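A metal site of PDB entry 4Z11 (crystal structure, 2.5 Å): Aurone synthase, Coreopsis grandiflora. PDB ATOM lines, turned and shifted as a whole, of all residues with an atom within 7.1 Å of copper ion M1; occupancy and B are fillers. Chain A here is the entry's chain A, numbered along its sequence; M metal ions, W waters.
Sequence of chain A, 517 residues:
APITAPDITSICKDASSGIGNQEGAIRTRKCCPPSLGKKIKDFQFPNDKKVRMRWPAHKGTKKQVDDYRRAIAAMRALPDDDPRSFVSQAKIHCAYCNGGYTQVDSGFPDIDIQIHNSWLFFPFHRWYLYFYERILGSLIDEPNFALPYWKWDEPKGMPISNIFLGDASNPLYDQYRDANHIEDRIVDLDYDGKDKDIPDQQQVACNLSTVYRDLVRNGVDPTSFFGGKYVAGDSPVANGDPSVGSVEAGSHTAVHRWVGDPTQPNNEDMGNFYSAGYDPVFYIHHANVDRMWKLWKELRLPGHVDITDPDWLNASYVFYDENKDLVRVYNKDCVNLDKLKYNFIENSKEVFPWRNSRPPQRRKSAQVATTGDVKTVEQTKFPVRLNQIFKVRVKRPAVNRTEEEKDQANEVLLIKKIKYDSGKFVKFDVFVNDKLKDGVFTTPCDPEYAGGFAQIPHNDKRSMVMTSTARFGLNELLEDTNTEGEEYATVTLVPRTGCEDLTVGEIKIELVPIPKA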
ATOM      1  N   HIS A  93     -29.220  -2.410 -13.811  1.00  0.00           N
ATOM      2  CA  HIS A  93     -28.228  -1.367 -13.649  1.00  0.00           C
ATOM      3  C   HIS A  93     -27.015  -1.642 -14.527  1.00  0.00           C
ATOM      4  O   HIS A  93     -26.446  -0.736 -15.122  1.00  0.00           O
ATOM      5  CB  HIS A  93     -27.824  -1.235 -12.182  1.00  0.00           C
ATOM      6  CG  HIS A  93     -27.096   0.033 -11.863  1.00  0.00           C
ATOM      7  ND1 HIS A  93     -25.764   0.069 -11.518  1.00  0.00           N
ATOM      8  CD2 HIS A  93     -27.517   1.318 -11.854  1.00  0.00           C
ATOM      9  CE1 HIS A  93     -25.397   1.316 -11.299  1.00  0.00           C
ATOM     10  NE2 HIS A  93     -26.444   2.094 -11.492  1.00  0.00           N
ATOM     11  N   HIS A 116     -25.658   7.276 -17.305  1.00  0.00           N
ATOM     12  CA  HIS A 116     -24.827   8.036 -16.389  1.00  0.00           C
ATOM     13  C   HIS A 116     -24.110   9.146 -17.148  1.00  0.00           C
ATOM     14  O   HIS A 116     -24.167   9.184 -18.383  1.00  0.00           O
ATOM     15  CB  HIS A 116     -23.808   7.126 -15.690  1.00  0.00           C
ATOM     16  CG  HIS A 116     -24.438   6.062 -14.845  1.00  0.00           C
ATOM     17  ND1 HIS A 116     -24.601   4.764 -15.293  1.00  0.00           N
ATOM     18  CD2 HIS A 116     -24.932   6.089 -13.585  1.00  0.00           C
ATOM     19  CE1 HIS A 116     -25.170   4.042 -14.341  1.00  0.00           C
ATOM     20  NE2 HIS A 116     -25.384   4.820 -13.295  1.00  0.00           N
ATOM     21  N   PHE A 121     -29.422  10.816 -15.835  1.00  0.00           N
ATOM     22  CA  PHE A 121     -29.039  10.208 -14.560  1.00  0.00           C
ATOM     23  C   PHE A 121     -30.187  10.143 -13.558  1.00  0.00           C
ATOM     24  O   PHE A 121     -30.550   9.055 -13.095  1.00  0.00           O
ATOM     25  CB  PHE A 121     -27.875  11.000 -13.948  1.00  0.00           C
ATOM     26  CG  PHE A 121     -27.530  10.583 -12.550  1.00  0.00           C
ATOM     27  CD1 PHE A 121     -26.847   9.398 -12.307  1.00  0.00           C
ATOM     28  CD2 PHE A 121     -27.890  11.383 -11.471  1.00  0.00           C
ATOM     29  CE1 PHE A 121     -26.529   9.022 -11.012  1.00  0.00           C
ATOM     30  CE2 PHE A 121     -27.571  11.008 -10.176  1.00  0.00           C
ATOM     31  CZ  PHE A 121     -26.891   9.827  -9.946  1.00  0.00           C
ATOM     32  N   HIS A 125     -32.886   6.541 -12.768  1.00  0.00           N
ATOM     33  CA  HIS A 125     -32.848   5.864 -11.482  1.00  0.00           C
ATOM     34  C   HIS A 125     -34.163   6.013 -10.717  1.00  0.00           C
ATOM     35  O   HIS A 125     -34.500   5.186  -9.873  1.00  0.00           O
ATOM     36  CB  HIS A 125     -31.691   6.397 -10.651  1.00  0.00           C
ATOM     37  CG  HIS A 125     -30.345   5.970 -11.157  1.00  0.00           C
ATOM     38  ND1 HIS A 125     -29.580   6.762 -11.995  1.00  0.00           N
ATOM     39  CD2 HIS A 125     -29.637   4.827 -10.979  1.00  0.00           C
ATOM     40  CE1 HIS A 125     -28.461   6.134 -12.285  1.00  0.00           C
ATOM     41  NE2 HIS A 125     -28.470   4.955 -11.679  1.00  0.00           N
ATOM     42  N   HIS A 252     -23.014  11.340  -4.541  1.00  0.00           N
ATOM     43  CA  HIS A 252     -23.472  10.079  -5.094  1.00  0.00           C
ATOM     44  C   HIS A 252     -22.304   9.122  -5.329  1.00  0.00           C
ATOM     45  O   HIS A 252     -22.325   7.974  -4.885  1.00  0.00           O
ATOM     46  CB  HIS A 252     -24.217  10.300  -6.412  1.00  0.00           C
ATOM     47  CG  HIS A 252     -24.435   9.057  -7.204  1.00  0.00           C
ATOM     48  ND1 HIS A 252     -23.731   8.770  -8.351  1.00  0.00           N
ATOM     49  CD2 HIS A 252     -25.294   8.018  -7.021  1.00  0.00           C
ATOM     50  CE1 HIS A 252     -24.134   7.609  -8.831  1.00  0.00           C
ATOM     51  NE2 HIS A 252     -25.080   7.135  -8.052  1.00  0.00           N
ATOM     52  N   THR A 253     -21.281   9.607  -6.026  1.00  0.00           N
ATOM     53  CA  THR A 253     -20.108   8.800  -6.345  1.00  0.00           C
ATOM     54  C   THR A 253     -19.365   8.408  -5.074  1.00  0.00           C
ATOM     55  O   THR A 253     -18.848   7.296  -4.967  1.00  0.00           O
ATOM     56  CB  THR A 253     -19.148   9.556  -7.298  1.00  0.00           C
ATOM     57  OG1 THR A 253     -19.738   9.648  -8.591  1.00  0.00           O
ATOM     58  CG2 THR A 253     -17.800   8.849  -7.404  1.00  0.00           C
ATOM     59  N   HIS A 256     -20.731   5.302  -3.351  1.00  0.00           N
ATOM     60  CA  HIS A 256     -20.418   4.098  -4.105  1.00  0.00           C
ATOM     61  C   HIS A 256     -19.029   3.568  -3.772  1.00  0.00           C
ATOM     62  O   HIS A 256     -18.856   2.377  -3.521  1.00  0.00           O
ATOM     63  CB  HIS A 256     -20.514   4.359  -5.617  1.00  0.00           C
ATOM     64  CG  HIS A 256     -21.906   4.241  -6.157  1.00  0.00           C
ATOM     65  ND1 HIS A 256     -22.493   3.032  -6.440  1.00  0.00           N
ATOM     66  CD2 HIS A 256     -22.821   5.196  -6.460  1.00  0.00           C
ATOM     67  CE1 HIS A 256     -23.718   3.235  -6.891  1.00  0.00           C
ATOM     68  NE2 HIS A 256     -23.943   4.536  -6.917  1.00  0.00           N
ATOM     69  N   MET A 270     -20.799  -2.252  -4.600  1.00  0.00           N
ATOM     70  CA  MET A 270     -21.186  -0.856  -4.808  1.00  0.00           C
ATOM     71  C   MET A 270     -20.162  -0.029  -5.585  1.00  0.00           C
ATOM     72  O   MET A 270     -20.517   0.962  -6.222  1.00  0.00           O
ATOM     73  CB  MET A 270     -21.431  -0.178  -3.458  1.00  0.00           C
ATOM     74  CG  MET A 270     -22.768  -0.520  -2.838  1.00  0.00           C
ATOM     75  SD  MET A 270     -24.127   0.417  -3.562  1.00  0.00           S
ATOM     76  CE  MET A 270     -23.864   2.038  -2.836  1.00  0.00           C
ATOM     77  N   PHE A 273     -20.557   0.138 -11.344  1.00  0.00           N
ATOM     78  CA  PHE A 273     -21.922   0.152 -11.863  1.00  0.00           C
ATOM     79  C   PHE A 273     -22.474  -1.249 -12.116  1.00  0.00           C
ATOM     80  O   PHE A 273     -23.638  -1.531 -11.824  1.00  0.00           O
ATOM     81  CB  PHE A 273     -21.990   0.945 -13.170  1.00  0.00           C
ATOM     82  CG  PHE A 273     -21.833   2.435 -13.009  1.00  0.00           C
ATOM     83  CD1 PHE A 273     -22.313   3.090 -11.886  1.00  0.00           C
ATOM     84  CD2 PHE A 273     -21.215   3.185 -14.005  1.00  0.00           C
ATOM     85  CE1 PHE A 273     -22.169   4.458 -11.745  1.00  0.00           C
ATOM     86  CE2 PHE A 273     -21.061   4.560 -13.870  1.00  0.00           C
ATOM     87  CZ  PHE A 273     -21.546   5.193 -12.747  1.00  0.00           C
ATOM     88  N   ALA A 276     -23.293  -2.955  -8.607  1.00  0.00           N
ATOM     89  CA  ALA A 276     -23.890  -2.180  -7.520  1.00  0.00           C
ATOM     90  C   ALA A 276     -25.257  -2.718  -7.113  1.00  0.00           C
ATOM     91  O   ALA A 276     -25.606  -2.705  -5.935  1.00  0.00           O
ATOM     92  CB  ALA A 276     -24.006  -0.717  -7.933  1.00  0.00           C
ATOM     93  N   PHE A 282     -27.709  -0.249  -2.315  1.00  0.00           N
ATOM     94  CA  PHE A 282     -27.636   0.522  -3.547  1.00  0.00           C
ATOM     95  C   PHE A 282     -28.935   1.252  -3.845  1.00  0.00           C
ATOM     96  O   PHE A 282     -28.934   2.451  -4.130  1.00  0.00           O
ATOM     97  CB  PHE A 282     -27.300  -0.395  -4.726  1.00  0.00           C
ATOM     98  CG  PHE A 282     -27.549   0.220  -6.067  1.00  0.00           C
ATOM     99  CD1 PHE A 282     -26.673   1.164  -6.586  1.00  0.00           C
ATOM    100  CD2 PHE A 282     -28.651  -0.139  -6.813  1.00  0.00           C
ATOM    101  CE1 PHE A 282     -26.905   1.741  -7.822  1.00  0.00           C
ATOM    102  CE2 PHE A 282     -28.886   0.434  -8.058  1.00  0.00           C
ATOM    103  CZ  PHE A 282     -28.014   1.379  -8.553  1.00  0.00           C
ATOM    104  N   HIS A 285     -29.604   3.891  -1.262  1.00  0.00           N
ATOM    105  CA  HIS A 285     -28.754   5.046  -1.509  1.00  0.00           C
ATOM    106  C   HIS A 285     -29.385   5.936  -2.578  1.00  0.00           C
ATOM    107  O   HIS A 285     -29.476   7.150  -2.415  1.00  0.00           O
ATOM    108  CB  HIS A 285     -27.353   4.595  -1.942  1.00  0.00           C
ATOM    109  CG  HIS A 285     -26.509   5.683  -2.516  1.00  0.00           C
ATOM    110  ND1 HIS A 285     -26.353   6.908  -1.903  1.00  0.00           N
ATOM    111  CD2 HIS A 285     -25.759   5.731  -3.640  1.00  0.00           C
ATOM    112  CE1 HIS A 285     -25.547   7.661  -2.632  1.00  0.00           C
ATOM    113  NE2 HIS A 285     -25.178   6.969  -3.696  1.00  0.00           N
ATOM    114  N   HIS A 286     -29.844   5.315  -3.666  1.00  0.00           N
ATOM    115  CA  HIS A 286     -30.450   6.047  -4.775  1.00  0.00           C
ATOM    116  C   HIS A 286     -31.832   6.570  -4.418  1.00  0.00           C
ATOM    117  O   HIS A 286     -32.357   7.463  -5.084  1.00  0.00           O
ATOM    118  CB  HIS A 286     -30.525   5.159  -6.010  1.00  0.00           C
ATOM    119  CG  HIS A 286     -29.277   5.181  -6.831  1.00  0.00           C
ATOM    120  ND1 HIS A 286     -29.120   5.985  -7.935  1.00  0.00           N
ATOM    121  CD2 HIS A 286     -28.102   4.528  -6.674  1.00  0.00           C
ATOM    122  CE1 HIS A 286     -27.915   5.809  -8.447  1.00  0.00           C
ATOM    123  NE2 HIS A 286     -27.272   4.922  -7.700  1.00  0.00           N
ATOM    124  N   VAL A 289     -30.808   9.899  -3.301  1.00  0.00           N
ATOM    125  CA  VAL A 289     -30.390  10.642  -4.487  1.00  0.00           C
ATOM    126  C   VAL A 289     -31.636  11.114  -5.232  1.00  0.00           C
ATOM    127  O   VAL A 289     -31.698  12.235  -5.726  1.00  0.00           O
ATOM    128  CB  VAL A 289     -29.501   9.818  -5.428  1.00  0.00           C
ATOM    129  CG1 VAL A 289     -29.252  10.535  -6.748  1.00  0.00           C
ATOM    130  CG2 VAL A 289     -28.173   9.486  -4.745  1.00  0.00           C
ATOM    131  N   ILE A 456     -16.662   7.210 -11.430  1.00  0.00           N
ATOM    132  CA  ILE A 456     -16.689   5.755 -11.365  1.00  0.00           C
ATOM    133  C   ILE A 456     -16.274   5.219 -12.730  1.00  0.00           C
ATOM    134  O   ILE A 456     -16.599   5.829 -13.747  1.00  0.00           O
ATOM    135  CB  ILE A 456     -18.085   5.238 -10.968  1.00  0.00           C
ATOM    136  CG1 ILE A 456     -18.406   5.651  -9.534  1.00  0.00           C
ATOM    137  CG2 ILE A 456     -18.189   3.722 -11.102  1.00  0.00           C
ATOM    138  CD1 ILE A 456     -19.854   5.487  -9.143  1.00  0.00           C
HETATM  139 CU    CU M   1     -25.371   5.158  -8.178  1.00  0.00          CU
HETATM  140 CU    CU M   2     -26.622   4.108 -11.814  1.00  0.00          CU
HETATM  141  O   HOH W   1     -25.054   4.704 -10.198  1.00  0.00           O
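A ring nitrogen (ND1) of His 256 is in hydrogen-bond range of the backbone carbonyl oxygen of Met 270 (2.9 Å).
NE2 of His 285 sits at hydrogen-bond distance from O of His 252, at 3.3 Å.
CE1 of Phe 282 touches copper ion M1 (3.8 Å).
Of the 15 residues printed, 4 come within 4 Å of copper ion M1.
Along chain A the residues within 4 Å of copper ion M1 span positions 252 to 286.
The nearest printed residue that does not touch copper ion M1 is His 285 (4.6 Å).
Copper ion M1 is bound by a ring nitrogen (NE2) of His 286 (2.0 Å), a ring nitrogen (NE2) of His 252 (2.0 Å), a ring nitrogen (NE2) of His 256 (2.0 Å) and water W1 (2.1 Å).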
